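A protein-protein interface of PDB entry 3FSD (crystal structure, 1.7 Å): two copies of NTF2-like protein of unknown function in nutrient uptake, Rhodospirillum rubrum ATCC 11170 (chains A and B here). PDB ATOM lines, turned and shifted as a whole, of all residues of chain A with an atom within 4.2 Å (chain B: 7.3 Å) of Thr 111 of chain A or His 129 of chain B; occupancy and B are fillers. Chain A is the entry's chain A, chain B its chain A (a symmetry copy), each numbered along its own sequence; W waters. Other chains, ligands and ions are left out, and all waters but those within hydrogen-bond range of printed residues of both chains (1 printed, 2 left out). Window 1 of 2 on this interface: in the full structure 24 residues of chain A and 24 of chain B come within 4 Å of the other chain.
Thr 111 of chain A touches His 129 of chain B, and with the chains exchanged His 129 of chain A touches Thr 111 of chain B. Ile 113 of chain A touches its own counterpart, Ile 113 of chain B. His 129 of chain B touches its own counterpart, His 129 of chain A. His 129 of chain A touches Ser 131 of chain B, and with the chains exchanged Ser 131 of chain A touches His 129 of chain B. Positions printed for both chains: 89, 109, 110, 111, 112, 113, 128, 129 and 131. Of the 17 pairs that touch across the chains among the printed residues, 9 have their exchanged pair printed and touching as well.
Water W1 lies within hydrogen-bond range of N of Val 52 of chain B (3.0 Å) and NH2 of Arg 109 of chain A (3.2 Å).
Hydrophobic or aromatic side chains of chain A that line the printed part of chain B: Val 88, Val 90, Ile 113 and His 129. Of the 22 printed residues of chain B, 9 touch a printed residue of chain A. Among the printed residues, no Asp or Glu carboxylate lies within 4 Å of a Lys or Arg side-chain nitrogen of the other chain.
The backbone NH (N) of Arg 109 of chain B sits at hydrogen-bond distance from the backbone carbonyl oxygen (O) of Ser 131 of chain B (2.8 Å). The backbone NH (N) of Ile 113 of chain B is in hydrogen-bond range of the backbone carbonyl oxygen (O) of Ala 127 of chain B, 2.8 Å away. The backbone NH (N) of Cys 130 of chain B is in hydrogen-bond range of the backbone carbonyl oxygen (O) of Val 46 of chain B, 3.0 Å away. The backbone NH (N) of Thr 111 of chain A is in hydrogen-bond range of the backbone carbonyl oxygen (O) of His 129 of chain A (2.8 Å). The backbone NH (N) of Arg 109 of chain A lies within hydrogen-bond range of the backbone carbonyl oxygen (O) of Ser 131 of chain A, 2.8 Å away. The backbone NH (N) of Gly 50 of chain B lies within hydrogen-bond range of the side-chain carboxylate (OD1) of Asp 47 of chain B, at 3.2 Å.
Of chain B, only Val 46 and His 129 come within 4 Å of Thr 111 of chain A. His 129 of chain B touches four residues of chain A. Of the printed residues of chain A, Val 52 of chain B touches Val 90 and Arg 109. Printed residues of chain A within 4 Å of Ile 113 of chain B: Val 88 and Ile 113. Printed residues of chain B within 4 Å of His 129 of chain A: Arg 109, Thr 111, His 129 and Ser 131. Printed residues of chain B within 4 Å of Val 90 of chain A: Val 46 (3.6 Å) and Val 52 (3.8 Å). Val 91 of chain B touches none of the printed residues of chain A. Val 89 of chain A touches none of the printed residues of chain B. The nearest residue of chain B that does not touch Thr 111 of chain A is Ile 113 of chain B (4.1 Å).
Val 88 of chain A touches Ile 113 of chain B (CG2 to CG2, 3.8 Å). Val 88 of chain A touches Ala 127 of chain B. Val 90 of chain A touches Val 46 of chain B. Val 52 of chain B touches Val 90 of chain A. Arg 109 of chain A touches Val 46 of chain B. Arg 109 of chain A touches Val 52 of chain B. His 129 of chain B touches Arg 109 of chain A. OG1 of Thr 111 of chain A touches CG2 of Val 46 of chain B, at 3.7 Å. CD2 of His 129 of chain A touches CD2 of His 129 of chain B, 3.4 Å away. Ser 131 of chain B touches Ser 131 of chain A.
The side-chain hydroxyl (OG1) of Thr 111 of chain A lies within hydrogen-bond range of a ring nitrogen (ND1) of His 129 of chain B, at 2.8 Å. O of Gly 50 of chain B is in hydrogen-bond range of NE of Arg 109 of chain A (2.7 Å). ND1 of His 129 of chain A is in hydrogen-bond range of OG1 of Thr 111 of chain B (2.8 Å). The side-chain hydroxyl (OG) of Ser 131 of chain A sits at hydrogen-bond distance from a ring nitrogen (NE2) of His 129 of chain B, at 2.8 Å. A ring nitrogen (NE2) of His 129 of chain A sits at hydrogen-bond distance from the side-chain hydroxyl of Ser 131 of chain B (2.8 Å).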
ATOM      1  N   VAL A  88      -1.821  15.164 -27.175  1.00  0.00           N
ATOM      2  CA  VAL A  88      -0.627  15.811 -26.574  1.00  0.00           C
ATOM      3  C   VAL A  88       0.473  15.909 -27.619  1.00  0.00           C
ATOM      4  O   VAL A  88       0.733  14.965 -28.325  1.00  0.00           O
ATOM      5  CB  VAL A  88      -0.082  15.046 -25.386  1.00  0.00           C
ATOM      6  CG1 VAL A  88       0.975  15.860 -24.687  1.00  0.00           C
ATOM      7  CG2 VAL A  88      -1.194  14.641 -24.436  1.00  0.00           C
ATOM      8  N   VAL A  89       1.097  17.079 -27.699  1.00  0.00           N
ATOM      9  CA  VAL A  89       2.242  17.331 -28.557  1.00  0.00           C
ATOM     10  C   VAL A  89       3.378  17.862 -27.677  1.00  0.00           C
ATOM     11  O   VAL A  89       3.213  18.788 -26.922  1.00  0.00           O
ATOM     12  CB  VAL A  89       1.930  18.295 -29.695  1.00  0.00           C
ATOM     13  CG1 VAL A  89       3.192  18.599 -30.509  1.00  0.00           C
ATOM     14  CG2 VAL A  89       0.776  17.733 -30.547  1.00  0.00           C
ATOM     15  N   VAL A  90       4.522  17.191 -27.740  1.00  0.00           N
ATOM     16  CA  VAL A  90       5.726  17.626 -26.961  1.00  0.00           C
ATOM     17  C   VAL A  90       6.787  17.891 -28.009  1.00  0.00           C
ATOM     18  O   VAL A  90       7.129  16.996 -28.765  1.00  0.00           O
ATOM     19  CB  VAL A  90       6.200  16.551 -25.941  1.00  0.00           C
ATOM     20  CG1 VAL A  90       7.569  16.951 -25.274  1.00  0.00           C
ATOM     21  CG2 VAL A  90       5.094  16.361 -24.880  1.00  0.00           C
ATOM     22  N   ARG A 109      11.176  23.592 -24.518  1.00  0.00           N
ATOM     23  CA  ARG A 109      10.336  22.437 -24.736  1.00  0.00           C
ATOM     24  C   ARG A 109       8.938  22.863 -24.471  1.00  0.00           C
ATOM     25  O   ARG A 109       8.644  23.456 -23.448  1.00  0.00           O
ATOM     26  CB  ARG A 109      10.685  21.293 -23.804  1.00  0.00           C
ATOM     27  CG  ARG A 109      10.054  19.930 -24.170  1.00  0.00           C
ATOM     28  CD  ARG A 109      10.775  19.196 -25.297  1.00  0.00           C
ATOM     29  NE  ARG A 109      12.140  18.865 -24.982  1.00  0.00           N
ATOM     30  CZ  ARG A 109      12.973  18.253 -25.808  1.00  0.00           C
ATOM     31  NH1 ARG A 109      12.535  17.889 -27.001  1.00  0.00           N
ATOM     32  NH2 ARG A 109      14.229  17.996 -25.430  1.00  0.00           N
ATOM     33  N   PHE A 110       8.075  22.573 -25.424  1.00  0.00           N
ATOM     34  CA  PHE A 110       6.666  22.835 -25.308  1.00  0.00           C
ATOM     35  C   PHE A 110       5.924  21.510 -25.162  1.00  0.00           C
ATOM     36  O   PHE A 110       6.212  20.499 -25.892  1.00  0.00           O
ATOM     37  CB  PHE A 110       6.075  23.495 -26.542  1.00  0.00           C
ATOM     38  CG  PHE A 110       6.345  24.946 -26.659  1.00  0.00           C
ATOM     39  CD1 PHE A 110       7.532  25.378 -27.206  1.00  0.00           C
ATOM     40  CD2 PHE A 110       5.412  25.882 -26.279  1.00  0.00           C
ATOM     41  CE1 PHE A 110       7.797  26.721 -27.385  1.00  0.00           C
ATOM     42  CE2 PHE A 110       5.683  27.220 -26.441  1.00  0.00           C
ATOM     43  CZ  PHE A 110       6.899  27.628 -27.001  1.00  0.00           C
ATOM     44  N   THR A 111       4.986  21.514 -24.219  1.00  0.00           N
ATOM     45  CA  THR A 111       3.922  20.498 -24.106  1.00  0.00           C
ATOM     46  C   THR A 111       2.599  21.204 -24.378  1.00  0.00           C
ATOM     47  O   THR A 111       2.314  22.238 -23.785  1.00  0.00           O
ATOM     48  CB  THR A 111       3.898  19.849 -22.701  1.00  0.00           C
ATOM     49  OG1 THR A 111       5.172  19.273 -22.441  1.00  0.00           O
ATOM     50  CG2 THR A 111       2.784  18.771 -22.546  1.00  0.00           C
ATOM     51  N   ARG A 112       1.810  20.671 -25.313  1.00  0.00           N
ATOM     52  CA  ARG A 112       0.548  21.226 -25.666  1.00  0.00           C
ATOM     53  C   ARG A 112      -0.505  20.144 -25.660  1.00  0.00           C
ATOM     54  O   ARG A 112      -0.255  19.027 -26.084  1.00  0.00           O
ATOM     55  CB  ARG A 112       0.614  21.860 -27.042  1.00  0.00           C
ATOM     56  CG  ARG A 112       1.009  23.331 -26.971  1.00  0.00           C
ATOM     57  CD  ARG A 112       0.916  23.990 -28.370  1.00  0.00           C
ATOM     58  NE  ARG A 112       1.965  23.514 -29.227  1.00  0.00           N
ATOM     59  CZ  ARG A 112       3.127  24.130 -29.405  1.00  0.00           C
ATOM     60  NH1 ARG A 112       3.377  25.270 -28.812  1.00  0.00           N
ATOM     61  NH2 ARG A 112       4.031  23.614 -30.219  1.00  0.00           N
ATOM     62  N   ILE A 113      -1.657  20.477 -25.131  1.00  0.00           N
ATOM     63  CA  ILE A 113      -2.804  19.589 -25.021  1.00  0.00           C
ATOM     64  C   ILE A 113      -3.983  20.203 -25.751  1.00  0.00           C
ATOM     65  O   ILE A 113      -4.467  21.293 -25.384  1.00  0.00           O
ATOM     66  CB  ILE A 113      -3.259  19.315 -23.568  1.00  0.00           C
ATOM     67  CG1 ILE A 113      -2.128  18.806 -22.689  1.00  0.00           C
ATOM     68  CG2 ILE A 113      -4.369  18.227 -23.640  1.00  0.00           C
ATOM     69  CD1 ILE A 113      -1.197  19.819 -22.110  1.00  0.00           C
ATOM     70  N   GLY A 128      -1.068  24.077 -21.994  1.00  0.00           N
ATOM     71  CA  GLY A 128       0.280  23.949 -22.429  1.00  0.00           C
ATOM     72  C   GLY A 128       1.255  24.375 -21.344  1.00  0.00           C
ATOM     73  O   GLY A 128       0.875  24.975 -20.341  1.00  0.00           O
ATOM     74  N   HIS A 129       2.518  24.073 -21.603  1.00  0.00           N
ATOM     75  CA  HIS A 129       3.619  24.334 -20.687  1.00  0.00           C
ATOM     76  C   HIS A 129       4.862  24.544 -21.559  1.00  0.00           C
ATOM     77  O   HIS A 129       5.165  23.727 -22.440  1.00  0.00           O
ATOM     78  CB  HIS A 129       3.806  23.102 -19.812  1.00  0.00           C
ATOM     79  CG  HIS A 129       4.619  23.292 -18.560  1.00  0.00           C
ATOM     80  ND1 HIS A 129       4.252  22.703 -17.372  1.00  0.00           N
ATOM     81  CD2 HIS A 129       5.792  23.917 -18.327  1.00  0.00           C
ATOM     82  CE1 HIS A 129       5.147  23.005 -16.447  1.00  0.00           C
ATOM     83  NE2 HIS A 129       6.099  23.739 -16.995  1.00  0.00           N
ATOM     84  N   SER A 131       9.177  25.408 -21.102  1.00  0.00           N
ATOM     85  CA  SER A 131      10.303  25.661 -20.207  1.00  0.00           C
ATOM     86  C   SER A 131      11.578  25.551 -21.012  1.00  0.00           C
ATOM     87  O   SER A 131      11.621  24.944 -22.054  1.00  0.00           O
ATOM     88  CB  SER A 131      10.283  24.682 -19.041  1.00  0.00           C
ATOM     89  OG  SER A 131      10.530  23.370 -19.435  1.00  0.00           O
ATOM     90  N   ALA B  44       5.301  10.271 -22.034  1.00  0.00           N
ATOM     91  CA  ALA B  44       6.305  11.255 -22.410  1.00  0.00           C
ATOM     92  C   ALA B  44       6.331  12.291 -21.315  1.00  0.00           C
ATOM     93  O   ALA B  44       5.351  13.020 -21.172  1.00  0.00           O
ATOM     94  CB  ALA B  44       5.891  11.898 -23.716  1.00  0.00           C
ATOM     95  N   PHE B  45       7.425  12.357 -20.561  1.00  0.00           N
ATOM     96  CA  PHE B  45       7.495  13.269 -19.391  1.00  0.00           C
ATOM     97  C   PHE B  45       8.665  14.209 -19.553  1.00  0.00           C
ATOM     98  O   PHE B  45       9.770  13.776 -19.731  1.00  0.00           O
ATOM     99  CB  PHE B  45       7.579  12.542 -18.048  1.00  0.00           C
ATOM    100  CG  PHE B  45       7.168  13.427 -16.889  1.00  0.00           C
ATOM    101  CD1 PHE B  45       8.056  14.327 -16.338  1.00  0.00           C
ATOM    102  CD2 PHE B  45       5.883  13.412 -16.412  1.00  0.00           C
ATOM    103  CE1 PHE B  45       7.685  15.145 -15.299  1.00  0.00           C
ATOM    104  CE2 PHE B  45       5.502  14.252 -15.366  1.00  0.00           C
ATOM    105  CZ  PHE B  45       6.408  15.129 -14.831  1.00  0.00           C
ATOM    106  N   VAL B  46       8.383  15.502 -19.581  1.00  0.00           N
ATOM    107  CA  VAL B  46       9.425  16.534 -19.689  1.00  0.00           C
ATOM    108  C   VAL B  46       9.899  16.890 -18.284  1.00  0.00           C
ATOM    109  O   VAL B  46       9.139  17.361 -17.444  1.00  0.00           O
ATOM    110  CB  VAL B  46       8.893  17.792 -20.391  1.00  0.00           C
ATOM    111  CG1 VAL B  46       9.988  18.825 -20.514  1.00  0.00           C
ATOM    112  CG2 VAL B  46       8.327  17.417 -21.778  1.00  0.00           C
ATOM    113  N   ASP B  47      11.171  16.737 -18.058  1.00  0.00           N
ATOM    114  CA  ASP B  47      11.756  17.027 -16.727  1.00  0.00           C
ATOM    115  C   ASP B  47      12.175  18.488 -16.598  1.00  0.00           C
ATOM    116  O   ASP B  47      11.975  19.300 -17.499  1.00  0.00           O
ATOM    117  CB  ASP B  47      12.889  16.047 -16.402  1.00  0.00           C
ATOM    118  CG  ASP B  47      14.198  16.355 -17.122  1.00  0.00           C
ATOM    119  OD1 ASP B  47      14.346  17.435 -17.738  1.00  0.00           O
ATOM    120  OD2 ASP B  47      15.085  15.484 -17.023  1.00  0.00           O
ATOM    121  N   HIS B  48      12.781  18.811 -15.459  1.00  0.00           N
ATOM    122  CA  HIS B  48      13.000  20.219 -15.147  1.00  0.00           C
ATOM    123  C   HIS B  48      14.137  20.847 -15.972  1.00  0.00           C
ATOM    124  O   HIS B  48      14.313  22.063 -15.936  1.00  0.00           O
ATOM    125  CB  HIS B  48      13.178  20.431 -13.635  1.00  0.00           C
ATOM    126  CG  HIS B  48      14.398  19.796 -13.054  1.00  0.00           C
ATOM    127  ND1 HIS B  48      14.706  19.904 -11.714  1.00  0.00           N
ATOM    128  CD2 HIS B  48      15.396  19.071 -13.610  1.00  0.00           C
ATOM    129  CE1 HIS B  48      15.838  19.267 -11.473  1.00  0.00           C
ATOM    130  NE2 HIS B  48      16.278  18.748 -12.604  1.00  0.00           N
ATOM    131  N   THR B  49      14.880  20.045 -16.734  1.00  0.00           N
ATOM    132  CA  THR B  49      15.845  20.596 -17.690  1.00  0.00           C
ATOM    133  C   THR B  49      15.343  20.609 -19.151  1.00  0.00           C
ATOM    134  O   THR B  49      16.100  20.904 -20.079  1.00  0.00           O
ATOM    135  CB  THR B  49      17.158  19.839 -17.640  1.00  0.00           C
ATOM    136  OG1 THR B  49      16.927  18.496 -18.049  1.00  0.00           O
ATOM    137  CG2 THR B  49      17.730  19.880 -16.216  1.00  0.00           C
ATOM    138  N   GLY B  50      14.072  20.238 -19.347  1.00  0.00           N
ATOM    139  CA  GLY B  50      13.465  20.133 -20.653  1.00  0.00           C
ATOM    140  C   GLY B  50      13.769  18.874 -21.439  1.00  0.00           C
ATOM    141  O   GLY B  50      13.503  18.842 -22.644  1.00  0.00           O
ATOM    142  N   VAL B  52      13.067  15.018 -22.459  1.00  0.00           N
ATOM    143  CA  VAL B  52      11.866  14.180 -22.570  1.00  0.00           C
ATOM    144  C   VAL B  52      12.223  12.777 -22.155  1.00  0.00           C
ATOM    145  O   VAL B  52      13.143  12.160 -22.744  1.00  0.00           O
ATOM    146  CB  VAL B  52      11.255  14.168 -23.987  1.00  0.00           C
ATOM    147  CG1 VAL B  52       9.896  13.407 -24.019  1.00  0.00           C
ATOM    148  CG2 VAL B  52      11.041  15.549 -24.491  1.00  0.00           C
ATOM    149  N   VAL B  89      -4.165  18.313 -15.449  1.00  0.00           N
ATOM    150  CA  VAL B  89      -3.992  18.830 -14.102  1.00  0.00           C
ATOM    151  C   VAL B  89      -2.730  19.698 -14.093  1.00  0.00           C
ATOM    152  O   VAL B  89      -1.678  19.289 -14.519  1.00  0.00           O
ATOM    153  CB  VAL B  89      -3.912  17.731 -13.050  1.00  0.00           C
ATOM    154  CG1 VAL B  89      -3.635  18.325 -11.666  1.00  0.00           C
ATOM    155  CG2 VAL B  89      -5.191  16.873 -13.100  1.00  0.00           C
ATOM    156  N   VAL B  91      -0.558  22.008 -11.439  1.00  0.00           N
ATOM    157  CA  VAL B  91      -0.499  22.160  -9.989  1.00  0.00           C
ATOM    158  C   VAL B  91       0.863  22.721  -9.544  1.00  0.00           C
ATOM    159  O   VAL B  91       1.892  22.471 -10.161  1.00  0.00           O
ATOM    160  CB  VAL B  91      -0.906  20.803  -9.305  1.00  0.00           C
ATOM    161  CG1 VAL B  91       0.116  19.650  -9.640  1.00  0.00           C
ATOM    162  CG2 VAL B  91      -1.135  21.002  -7.807  1.00  0.00           C
ATOM    163  N   LEU B 108       8.044  23.513  -7.985  1.00  0.00           N
ATOM    164  CA  LEU B 108       7.769  23.239  -9.408  1.00  0.00           C
ATOM    165  C   LEU B 108       6.334  23.426  -9.787  1.00  0.00           C
ATOM    166  O   LEU B 108       5.422  23.315  -8.962  1.00  0.00           O
ATOM    167  CB  LEU B 108       8.142  21.798  -9.753  1.00  0.00           C
ATOM    168  CG  LEU B 108       9.587  21.375  -9.493  1.00  0.00           C
ATOM    169  CD1 LEU B 108       9.553  20.162  -8.607  1.00  0.00           C
ATOM    170  CD2 LEU B 108      10.354  21.115 -10.773  1.00  0.00           C
ATOM    171  N   ARG B 109       6.135  23.688 -11.073  1.00  0.00           N
ATOM    172  CA  ARG B 109       4.817  23.584 -11.656  1.00  0.00           C
ATOM    173  C   ARG B 109       4.793  22.328 -12.448  1.00  0.00           C
ATOM    174  O   ARG B 109       5.670  22.076 -13.255  1.00  0.00           O
ATOM    175  CB  ARG B 109       4.504  24.750 -12.574  1.00  0.00           C
ATOM    176  CG  ARG B 109       3.022  24.879 -12.992  1.00  0.00           C
ATOM    177  CD  ARG B 109       2.132  25.515 -11.927  1.00  0.00           C
ATOM    178  NE  ARG B 109       2.511  26.863 -11.597  1.00  0.00           N
ATOM    179  CZ  ARG B 109       1.908  27.610 -10.685  1.00  0.00           C
ATOM    180  NH1 ARG B 109       0.867  27.110 -10.040  1.00  0.00           N
ATOM    181  NH2 ARG B 109       2.338  28.850 -10.438  1.00  0.00           N
ATOM    182  N   PHE B 110       3.780  21.525 -12.191  1.00  0.00           N
ATOM    183  CA  PHE B 110       3.547  20.305 -12.916  1.00  0.00           C
ATOM    184  C   PHE B 110       2.313  20.476 -13.795  1.00  0.00           C
ATOM    185  O   PHE B 110       1.250  21.035 -13.352  1.00  0.00           O
ATOM    186  CB  PHE B 110       3.240  19.120 -12.014  1.00  0.00           C
ATOM    187  CG  PHE B 110       4.423  18.517 -11.359  1.00  0.00           C
ATOM    188  CD1 PHE B 110       4.908  19.061 -10.191  1.00  0.00           C
ATOM    189  CD2 PHE B 110       5.022  17.386 -11.863  1.00  0.00           C
ATOM    190  CE1 PHE B 110       5.973  18.494  -9.520  1.00  0.00           C
ATOM    191  CE2 PHE B 110       6.093  16.831 -11.203  1.00  0.00           C
ATOM    192  CZ  PHE B 110       6.564  17.408 -10.018  1.00  0.00           C
ATOM    193  N   THR B 111       2.458  20.010 -15.031  1.00  0.00           N
ATOM    194  CA  THR B 111       1.335  19.751 -15.955  1.00  0.00           C
ATOM    195  C   THR B 111       1.289  18.245 -16.190  1.00  0.00           C
ATOM    196  O   THR B 111       2.302  17.636 -16.514  1.00  0.00           O
ATOM    197  CB  THR B 111       1.520  20.493 -17.300  1.00  0.00           C
ATOM    198  OG1 THR B 111       1.645  21.886 -17.042  1.00  0.00           O
ATOM    199  CG2 THR B 111       0.353  20.241 -18.301  1.00  0.00           C
ATOM    200  N   ARG B 112       0.120  17.637 -15.981  1.00  0.00           N
ATOM    201  CA  ARG B 112      -0.065  16.238 -16.166  1.00  0.00           C
ATOM    202  C   ARG B 112      -1.288  15.992 -17.015  1.00  0.00           C
ATOM    203  O   ARG B 112      -2.294  16.667 -16.872  1.00  0.00           O
ATOM    204  CB  ARG B 112      -0.232  15.545 -14.826  1.00  0.00           C
ATOM    205  CG  ARG B 112       1.105  15.084 -14.255  1.00  0.00           C
ATOM    206  CD  ARG B 112       0.891  14.246 -12.971  1.00  0.00           C
ATOM    207  NE  ARG B 112       0.455  15.080 -11.886  1.00  0.00           N
ATOM    208  CZ  ARG B 112       1.263  15.613 -10.977  1.00  0.00           C
ATOM    209  NH1 ARG B 112       2.550  15.369 -11.001  1.00  0.00           N
ATOM    210  NH2 ARG B 112       0.767  16.366 -10.012  1.00  0.00           N
ATOM    211  N   ILE B 113      -1.167  15.057 -17.926  1.00  0.00           N
ATOM    212  CA  ILE B 113      -2.218  14.663 -18.852  1.00  0.00           C
ATOM    213  C   ILE B 113      -2.516  13.187 -18.668  1.00  0.00           C
ATOM    214  O   ILE B 113      -1.642  12.325 -18.892  1.00  0.00           O
ATOM    215  CB  ILE B 113      -1.866  14.877 -20.342  1.00  0.00           C
ATOM    216  CG1 ILE B 113      -1.427  16.301 -20.639  1.00  0.00           C
ATOM    217  CG2 ILE B 113      -3.154  14.567 -21.159  1.00  0.00           C
ATOM    218  CD1 ILE B 113      -0.008  16.660 -20.347  1.00  0.00           C
ATOM    219  N   LEU B 125      -1.400   8.126 -16.549  1.00  0.00           N
ATOM    220  CA  LEU B 125      -0.692   9.312 -16.957  1.00  0.00           C
ATOM    221  C   LEU B 125      -0.040   9.076 -18.294  1.00  0.00           C
ATOM    222  O   LEU B 125       0.771   8.188 -18.436  1.00  0.00           O
ATOM    223  CB  LEU B 125       0.359   9.683 -15.901  1.00  0.00           C
ATOM    224  CG  LEU B 125       0.974  11.066 -16.120  1.00  0.00           C
ATOM    225  CD1 LEU B 125      -0.098  12.156 -15.940  1.00  0.00           C
ATOM    226  CD2 LEU B 125       2.197  11.217 -15.159  1.00  0.00           C
ATOM    227  N   ALA B 127       1.215  11.896 -20.258  1.00  0.00           N
ATOM    228  CA  ALA B 127       2.288  12.890 -20.405  1.00  0.00           C
ATOM    229  C   ALA B 127       2.319  13.850 -19.257  1.00  0.00           C
ATOM    230  O   ALA B 127       1.386  14.008 -18.491  1.00  0.00           O
ATOM    231  CB  ALA B 127       2.178  13.633 -21.753  1.00  0.00           C
ATOM    232  N   GLY B 128       3.458  14.499 -19.131  1.00  0.00           N
ATOM    233  CA  GLY B 128       3.615  15.504 -18.137  1.00  0.00           C
ATOM    234  C   GLY B 128       4.840  16.362 -18.407  1.00  0.00           C
ATOM    235  O   GLY B 128       5.683  16.032 -19.238  1.00  0.00           O
ATOM    236  N   HIS B 129       4.918  17.446 -17.651  1.00  0.00           N
ATOM    237  CA  HIS B 129       5.972  18.443 -17.767  1.00  0.00           C
ATOM    238  C   HIS B 129       6.140  19.055 -16.372  1.00  0.00           C
ATOM    239  O   HIS B 129       5.160  19.478 -15.742  1.00  0.00           O
ATOM    240  CB  HIS B 129       5.505  19.511 -18.746  1.00  0.00           C
ATOM    241  CG  HIS B 129       6.571  20.417 -19.301  1.00  0.00           C
ATOM    242  ND1 HIS B 129       6.573  20.793 -20.625  1.00  0.00           N
ATOM    243  CD2 HIS B 129       7.596  21.074 -18.719  1.00  0.00           C
ATOM    244  CE1 HIS B 129       7.591  21.608 -20.840  1.00  0.00           C
ATOM    245  NE2 HIS B 129       8.232  21.802 -19.702  1.00  0.00           N
ATOM    246  N   CYS B 130       7.373  19.185 -15.931  1.00  0.00           N
ATOM    247  CA  CYS B 130       7.633  19.952 -14.719  1.00  0.00           C
ATOM    248  C   CYS B 130       8.732  20.950 -14.938  1.00  0.00           C
ATOM    249  O   CYS B 130       9.693  20.668 -15.669  1.00  0.00           O
ATOM    250  CB  CYS B 130       7.987  19.019 -13.567  1.00  0.00           C
ATOM    251  SG  CYS B 130       9.608  18.258 -13.652  1.00  0.00           S
ATOM    252  N   SER B 131       8.577  22.130 -14.326  1.00  0.00           N
ATOM    253  CA  SER B 131       9.623  23.144 -14.415  1.00  0.00           C
ATOM    254  C   SER B 131       9.583  23.975 -13.152  1.00  0.00           C
ATOM    255  O   SER B 131       8.596  24.032 -12.460  1.00  0.00           O
ATOM    256  CB  SER B 131       9.428  23.999 -15.660  1.00  0.00           C
ATOM    257  OG  SER B 131       8.283  24.786 -15.600  1.00  0.00           O
HETATM  258  O   HOH W   1      15.038  15.038 -24.664  1.00  0.00           O
